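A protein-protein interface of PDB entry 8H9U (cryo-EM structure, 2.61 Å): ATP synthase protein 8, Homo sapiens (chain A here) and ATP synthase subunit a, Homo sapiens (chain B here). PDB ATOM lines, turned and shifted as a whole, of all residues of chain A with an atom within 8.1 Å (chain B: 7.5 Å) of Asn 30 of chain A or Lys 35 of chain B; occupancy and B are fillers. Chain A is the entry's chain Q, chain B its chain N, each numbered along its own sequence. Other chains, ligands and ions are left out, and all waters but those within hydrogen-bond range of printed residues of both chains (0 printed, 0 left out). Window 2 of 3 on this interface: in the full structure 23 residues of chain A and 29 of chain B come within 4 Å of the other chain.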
ATOM      1  N   ILE A  23     -14.220 -16.695   8.140  1.00  0.00           N
ATOM      2  CA  ILE A  23     -13.981 -15.261   8.240  1.00  0.00           C
ATOM      3  C   ILE A  23     -13.676 -14.854   9.672  1.00  0.00           C
ATOM      4  O   ILE A  23     -12.617 -14.285   9.953  1.00  0.00           O
ATOM      5  CB  ILE A  23     -15.176 -14.477   7.682  1.00  0.00           C
ATOM      6  CG1 ILE A  23     -15.275 -14.674   6.175  1.00  0.00           C
ATOM      7  CG2 ILE A  23     -15.025 -13.013   8.000  1.00  0.00           C
ATOM      8  CD1 ILE A  23     -16.457 -13.988   5.558  1.00  0.00           C
ATOM      9  N   THR A  24     -14.602 -15.116  10.594  1.00  0.00           N
ATOM     10  CA  THR A  24     -14.399 -14.701  11.978  1.00  0.00           C
ATOM     11  C   THR A  24     -13.121 -15.293  12.551  1.00  0.00           C
ATOM     12  O   THR A  24     -12.357 -14.600  13.230  1.00  0.00           O
ATOM     13  CB  THR A  24     -15.596 -15.103  12.827  1.00  0.00           C
ATOM     14  OG1 THR A  24     -16.798 -14.825  12.106  1.00  0.00           O
ATOM     15  CG2 THR A  24     -15.601 -14.318  14.113  1.00  0.00           C
ATOM     16  N   GLN A  25     -12.873 -16.577  12.294  1.00  0.00           N
ATOM     17  CA  GLN A  25     -11.608 -17.172  12.698  1.00  0.00           C
ATOM     18  C   GLN A  25     -10.434 -16.397  12.120  1.00  0.00           C
ATOM     19  O   GLN A  25      -9.415 -16.208  12.791  1.00  0.00           O
ATOM     20  CB  GLN A  25     -11.554 -18.629  12.256  1.00  0.00           C
ATOM     21  CG  GLN A  25     -12.542 -19.517  12.963  1.00  0.00           C
ATOM     22  CD  GLN A  25     -12.030 -20.926  13.106  1.00  0.00           C
ATOM     23  OE1 GLN A  25     -11.114 -21.341  12.400  1.00  0.00           O
ATOM     24  NE2 GLN A  25     -12.612 -21.673  14.032  1.00  0.00           N
ATOM     25  N   LEU A  26     -10.572 -15.918  10.886  1.00  0.00           N
ATOM     26  CA  LEU A  26      -9.482 -15.194  10.248  1.00  0.00           C
ATOM     27  C   LEU A  26      -9.293 -13.816  10.863  1.00  0.00           C
ATOM     28  O   LEU A  26      -8.294 -13.146  10.589  1.00  0.00           O
ATOM     29  CB  LEU A  26      -9.749 -15.096   8.748  1.00  0.00           C
ATOM     30  CG  LEU A  26      -8.652 -14.617   7.813  1.00  0.00           C
ATOM     31  CD1 LEU A  26      -8.629 -15.487   6.578  1.00  0.00           C
ATOM     32  CD2 LEU A  26      -8.910 -13.174   7.442  1.00  0.00           C
ATOM     33  N   LYS A  27     -10.230 -13.376  11.700  1.00  0.00           N
ATOM     34  CA  LYS A  27     -10.052 -12.113  12.401  1.00  0.00           C
ATOM     35  C   LYS A  27      -9.498 -12.315  13.801  1.00  0.00           C
ATOM     36  O   LYS A  27      -8.867 -11.406  14.347  1.00  0.00           O
ATOM     37  CB  LYS A  27     -11.372 -11.352  12.462  1.00  0.00           C
ATOM     38  CG  LYS A  27     -11.731 -10.681  11.161  1.00  0.00           C
ATOM     39  CD  LYS A  27     -13.057  -9.973  11.257  1.00  0.00           C
ATOM     40  CE  LYS A  27     -13.526  -9.537   9.889  1.00  0.00           C
ATOM     41  NZ  LYS A  27     -12.545  -8.629   9.242  1.00  0.00           N
ATOM     42  N   MET A  28      -9.718 -13.486  14.397  1.00  0.00           N
ATOM     43  CA  MET A  28      -9.104 -13.765  15.688  1.00  0.00           C
ATOM     44  C   MET A  28      -7.607 -13.996  15.541  1.00  0.00           C
ATOM     45  O   MET A  28      -6.819 -13.533  16.373  1.00  0.00           O
ATOM     46  CB  MET A  28      -9.776 -14.968  16.342  1.00  0.00           C
ATOM     47  CG  MET A  28     -11.189 -14.715  16.799  1.00  0.00           C
ATOM     48  SD  MET A  28     -11.306 -13.315  17.915  1.00  0.00           S
ATOM     49  CE  MET A  28     -12.150 -12.144  16.865  1.00  0.00           C
ATOM     50  N   LEU A  29      -7.197 -14.718  14.494  1.00  0.00           N
ATOM     51  CA  LEU A  29      -5.774 -14.863  14.206  1.00  0.00           C
ATOM     52  C   LEU A  29      -5.089 -13.514  14.114  1.00  0.00           C
ATOM     53  O   LEU A  29      -3.906 -13.392  14.448  1.00  0.00           O
ATOM     54  CB  LEU A  29      -5.574 -15.630  12.903  1.00  0.00           C
ATOM     55  CG  LEU A  29      -6.188 -17.018  12.849  1.00  0.00           C
ATOM     56  CD1 LEU A  29      -6.222 -17.492  11.419  1.00  0.00           C
ATOM     57  CD2 LEU A  29      -5.379 -17.956  13.704  1.00  0.00           C
ATOM     58  N   ASN A  30      -5.810 -12.498  13.666  1.00  0.00           N
ATOM     59  CA  ASN A  30      -5.279 -11.154  13.561  1.00  0.00           C
ATOM     60  C   ASN A  30      -5.453 -10.374  14.859  1.00  0.00           C
ATOM     61  O   ASN A  30      -5.253  -9.156  14.872  1.00  0.00           O
ATOM     62  CB  ASN A  30      -5.947 -10.433  12.395  1.00  0.00           C
ATOM     63  CG  ASN A  30      -5.146  -9.259  11.896  1.00  0.00           C
ATOM     64  OD1 ASN A  30      -4.092  -8.930  12.439  1.00  0.00           O
ATOM     65  ND2 ASN A  30      -5.628  -8.631  10.834  1.00  0.00           N
ATOM     66  N   THR A  31      -5.830 -11.050  15.943  1.00  0.00           N
ATOM     67  CA  THR A  31      -5.868 -10.467  17.285  1.00  0.00           C
ATOM     68  C   THR A  31      -4.869 -11.248  18.133  1.00  0.00           C
ATOM     69  O   THR A  31      -5.213 -12.228  18.793  1.00  0.00           O
ATOM     70  CB  THR A  31      -7.270 -10.524  17.877  1.00  0.00           C
ATOM     71  OG1 THR A  31      -8.146  -9.697  17.105  1.00  0.00           O
ATOM     72  CG2 THR A  31      -7.270 -10.020  19.307  1.00  0.00           C
ATOM     73  N   ASN A  32      -3.615 -10.819  18.098  1.00  0.00           N
ATOM     74  CA  ASN A  32      -2.538 -11.505  18.790  1.00  0.00           C
ATOM     75  C   ASN A  32      -2.217 -10.775  20.083  1.00  0.00           C
ATOM     76  O   ASN A  32      -2.440  -9.566  20.195  1.00  0.00           O
ATOM     77  CB  ASN A  32      -1.298 -11.580  17.909  1.00  0.00           C
ATOM     78  CG  ASN A  32      -1.001 -10.266  17.244  1.00  0.00           C
ATOM     79  OD1 ASN A  32      -1.724  -9.293  17.438  1.00  0.00           O
ATOM     80  ND2 ASN A  32       0.062 -10.222  16.453  1.00  0.00           N
ATOM     81  N   TYR A  33      -1.712 -11.536  21.061  1.00  0.00           N
ATOM     82  CA  TYR A  33      -1.340 -10.957  22.376  1.00  0.00           C
ATOM     83  C   TYR A  33       0.152 -11.209  22.606  1.00  0.00           C
ATOM     84  O   TYR A  33       0.539 -12.377  22.781  1.00  0.00           O
ATOM     85  CB  TYR A  33      -2.217 -11.556  23.477  1.00  0.00           C
ATOM     86  CG  TYR A  33      -3.695 -11.323  23.293  1.00  0.00           C
ATOM     87  CD1 TYR A  33      -4.229 -10.045  23.328  1.00  0.00           C
ATOM     88  CD2 TYR A  33      -4.563 -12.378  23.059  1.00  0.00           C
ATOM     89  CE1 TYR A  33      -5.584  -9.822  23.156  1.00  0.00           C
ATOM     90  CE2 TYR A  33      -5.922 -12.172  22.884  1.00  0.00           C
ATOM     91  CZ  TYR A  33      -6.436 -10.889  22.932  1.00  0.00           C
ATOM     92  OH  TYR A  33      -7.781 -10.676  22.757  1.00  0.00           O
ATOM     93  N   PRO B  32     -13.070  -5.162  13.472  1.00  0.00           N
ATOM     94  CA  PRO B  32     -11.864  -4.803  12.733  1.00  0.00           C
ATOM     95  C   PRO B  32     -10.631  -5.315  13.455  1.00  0.00           C
ATOM     96  O   PRO B  32     -10.646  -5.594  14.655  1.00  0.00           O
ATOM     97  CB  PRO B  32     -11.903  -3.275  12.703  1.00  0.00           C
ATOM     98  CG  PRO B  32     -12.752  -2.904  13.851  1.00  0.00           C
ATOM     99  CD  PRO B  32     -13.762  -3.983  14.009  1.00  0.00           C
ATOM    100  N   THR B  33      -9.554  -5.460  12.698  1.00  0.00           N
ATOM    101  CA  THR B  33      -8.296  -5.938  13.238  1.00  0.00           C
ATOM    102  C   THR B  33      -7.180  -5.023  12.766  1.00  0.00           C
ATOM    103  O   THR B  33      -7.308  -4.327  11.758  1.00  0.00           O
ATOM    104  CB  THR B  33      -8.019  -7.376  12.810  1.00  0.00           C
ATOM    105  OG1 THR B  33      -8.278  -7.512  11.408  1.00  0.00           O
ATOM    106  CG2 THR B  33      -8.910  -8.325  13.576  1.00  0.00           C
ATOM    107  N   SER B  34      -6.074  -5.030  13.503  1.00  0.00           N
ATOM    108  CA  SER B  34      -4.977  -4.133  13.184  1.00  0.00           C
ATOM    109  C   SER B  34      -3.660  -4.764  13.589  1.00  0.00           C
ATOM    110  O   SER B  34      -3.519  -5.260  14.710  1.00  0.00           O
ATOM    111  CB  SER B  34      -5.145  -2.785  13.887  1.00  0.00           C
ATOM    112  OG  SER B  34      -4.975  -2.925  15.285  1.00  0.00           O
ATOM    113  N   LYS B  35      -2.696  -4.736  12.671  1.00  0.00           N
ATOM    114  CA  LYS B  35      -1.325  -5.068  13.019  1.00  0.00           C
ATOM    115  C   LYS B  35      -0.755  -4.120  14.059  1.00  0.00           C
ATOM    116  O   LYS B  35       0.283  -4.428  14.654  1.00  0.00           O
ATOM    117  CB  LYS B  35      -0.435  -5.042  11.773  1.00  0.00           C
ATOM    118  CG  LYS B  35      -0.859  -5.993  10.669  1.00  0.00           C
ATOM    119  CD  LYS B  35      -0.802  -7.439  11.130  1.00  0.00           C
ATOM    120  CE  LYS B  35      -1.558  -8.339  10.173  1.00  0.00           C
ATOM    121  NZ  LYS B  35      -2.772  -7.665   9.639  1.00  0.00           N
ATOM    122  N   TYR B  36      -1.409  -2.986  14.293  1.00  0.00           N
ATOM    123  CA  TYR B  36      -0.892  -1.976  15.194  1.00  0.00           C
ATOM    124  C   TYR B  36      -0.833  -2.507  16.619  1.00  0.00           C
ATOM    125  O   TYR B  36      -1.503  -3.474  16.988  1.00  0.00           O
ATOM    126  CB  TYR B  36      -1.751  -0.718  15.140  1.00  0.00           C
ATOM    127  CG  TYR B  36      -1.464   0.144  13.943  1.00  0.00           C
ATOM    128  CD1 TYR B  36      -2.051   1.387  13.805  1.00  0.00           C
ATOM    129  CD2 TYR B  36      -0.604  -0.290  12.947  1.00  0.00           C
ATOM    130  CE1 TYR B  36      -1.789   2.176  12.709  1.00  0.00           C
ATOM    131  CE2 TYR B  36      -0.335   0.491  11.848  1.00  0.00           C
ATOM    132  CZ  TYR B  36      -0.930   1.724  11.734  1.00  0.00           C
ATOM    133  OH  TYR B  36      -0.669   2.512  10.639  1.00  0.00           O
ATOM    134  N   LEU B  37      -0.006  -1.852  17.424  1.00  0.00           N
ATOM    135  CA  LEU B  37       0.198  -2.238  18.809  1.00  0.00           C
ATOM    136  C   LEU B  37      -0.629  -1.414  19.780  1.00  0.00           C
ATOM    137  O   LEU B  37      -0.999  -1.916  20.845  1.00  0.00           O
ATOM    138  CB  LEU B  37       1.683  -2.125  19.157  1.00  0.00           C
ATOM    139  CG  LEU B  37       2.130  -2.313  20.594  1.00  0.00           C
ATOM    140  CD1 LEU B  37       3.408  -3.107  20.619  1.00  0.00           C
ATOM    141  CD2 LEU B  37       2.351  -0.948  21.177  1.00  0.00           C
ATOM    142  N   ILE B  38      -0.926  -0.166  19.437  1.00  0.00           N
ATOM    143  CA  ILE B  38      -1.890   0.655  20.158  1.00  0.00           C
ATOM    144  C   ILE B  38      -2.854   1.197  19.116  1.00  0.00           C
ATOM    145  O   ILE B  38      -2.437   1.902  18.189  1.00  0.00           O
ATOM    146  CB  ILE B  38      -1.226   1.795  20.935  1.00  0.00           C
ATOM    147  CG1 ILE B  38      -0.396   1.238  22.085  1.00  0.00           C
ATOM    148  CG2 ILE B  38      -2.274   2.756  21.457  1.00  0.00           C
ATOM    149  CD1 ILE B  38       0.455   2.278  22.761  1.00  0.00           C
ATOM    150  N   ASN B  39      -4.137   0.872  19.260  1.00  0.00           N
ATOM    151  CA  ASN B  39      -5.101   1.179  18.212  1.00  0.00           C
ATOM    152  C   ASN B  39      -6.388   1.777  18.764  1.00  0.00           C
ATOM    153  O   ASN B  39      -6.467   2.110  19.950  1.00  0.00           O
ATOM    154  CB  ASN B  39      -5.374  -0.079  17.389  1.00  0.00           C
ATOM    155  CG  ASN B  39      -5.780  -1.243  18.244  1.00  0.00           C
ATOM    156  OD1 ASN B  39      -6.018  -1.092  19.439  1.00  0.00           O
ATOM    157  ND2 ASN B  39      -5.828  -2.425  17.648  1.00  0.00           N
ATOM    158  N   ILE B  43     -11.332  -1.462  18.566  1.00  0.00           N
ATOM    159  CA  ILE B  43     -10.479  -2.637  18.654  1.00  0.00           C
ATOM    160  C   ILE B  43      -9.838  -2.735  20.026  1.00  0.00           C
ATOM    161  O   ILE B  43      -9.447  -3.824  20.456  1.00  0.00           O
ATOM    162  CB  ILE B  43      -9.423  -2.623  17.543  1.00  0.00           C
ATOM    163  CG1 ILE B  43     -10.069  -2.283  16.211  1.00  0.00           C
ATOM    164  CG2 ILE B  43      -8.777  -3.977  17.422  1.00  0.00           C
ATOM    165  CD1 ILE B  43      -9.075  -2.068  15.115  1.00  0.00           C
ATOM    166  N   GLN B  47     -10.464  -6.109  21.786  1.00  0.00           N
ATOM    167  CA  GLN B  47      -9.263  -6.937  21.988  1.00  0.00           C
ATOM    168  C   GLN B  47      -9.266  -7.315  23.456  1.00  0.00           C
ATOM    169  O   GLN B  47      -8.769  -8.390  23.793  1.00  0.00           O
ATOM    170  CB  GLN B  47      -8.004  -6.173  21.603  1.00  0.00           C
ATOM    171  CG  GLN B  47      -7.673  -6.265  20.128  1.00  0.00           C
ATOM    172  CD  GLN B  47      -6.221  -5.937  19.902  1.00  0.00           C
ATOM    173  OE1 GLN B  47      -5.480  -5.658  20.841  1.00  0.00           O
ATOM    174  NE2 GLN B  47      -5.802  -5.981  18.648  1.00  0.00           N
ATOM    175  N   LEU B  70      -9.168 -20.856  19.248  1.00  0.00           N
ATOM    176  CA  LEU B  70      -9.621 -19.995  18.165  1.00  0.00           C
ATOM    177  C   LEU B  70     -11.089 -20.241  17.863  1.00  0.00           C
ATOM    178  O   LEU B  70     -11.877 -19.300  17.740  1.00  0.00           O
ATOM    179  CB  LEU B  70      -8.777 -20.233  16.920  1.00  0.00           C
ATOM    180  CG  LEU B  70      -9.115 -19.321  15.749  1.00  0.00           C
ATOM    181  CD1 LEU B  70      -8.293 -18.072  15.841  1.00  0.00           C
ATOM    182  CD2 LEU B  70      -8.860 -20.026  14.440  1.00  0.00           C
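Gln 25 of chain A touches Leu 70 of chain B (OE1 to CD2, 3.3 Å).
Lys 27 of chain A touches Thr 33 of chain B.
CB of Met 28 of chain A touches CD1 of Leu 70 of chain B (3.5 Å).
Leu 29 of chain A touches Leu 70 of chain B (CD2 to CD1, 3.6 Å).
CG2 of Thr 33 of chain B touches OG1 of Thr 31 of chain A (3.9 Å).
Thr 31 of chain A touches Gln 47 of chain B.
Of the 11 printed residues of chain B, 4 touch a printed residue of chain A.
Of the 11 printed residues of chain A, 7 touch a printed residue of chain B.
Printed residues of chain A that touch a printed residue of chain B: Gln 25, Lys 27, Met 28, Leu 29, Asn 30, Thr 31 and Tyr 33.
Along chain A the printed residues that touch a printed residue of chain B span positions 25 to 33.
Among the printed residues, 9 pairs touch across the chains.
Of chain B, only Thr 33 and Lys 35 come within 4 Å of Asn 30 of chain A.
Lys 35 of chain B touches just one residue of chain A: Asn 30 (3.2 Å).
No residue of chain A comes within 4 Å of Ser 34 of chain B.
Of the printed residues of chain B, Leu 29 of chain A touches Leu 70 (3.6 Å).
Of the printed residues of chain A, Thr 33 of chain B touches Lys 27 (3.2 Å), Asn 30 (2.9 Å) and Thr 31 (3.9 Å).
Of the printed residues of chain B, Thr 31 of chain A touches Thr 33 (3.9 Å) and Gln 47 (3.9 Å).
Pro 32 of chain B touches none of the printed residues of chain A.
The nearest residue of chain B that does not touch Asn 30 of chain A is Ser 34 of chain B (4.3 Å).
The nearest residue of chain A that does not touch Lys 35 of chain B is Asn 32 of chain A (6.0 Å).
The side-chain hydroxyl of Thr 33 of chain B is in hydrogen-bond range of the side-chain amide nitrogen of Asn 30 of chain A (2.9 Å).
The side-chain amino group (NZ) of Lys 35 of chain B lies close to the side-chain amide nitrogen (ND2) of Asn 30 of chain A, 3.2 Å away.
O of Gln 47 of chain B sits at hydrogen-bond distance from OH of Tyr 33 of chain A.
The side-chain hydroxyl (OG1) of Thr 31 of chain A sits at hydrogen-bond distance from the backbone carbonyl oxygen (O) of Lys 27 of chain A.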
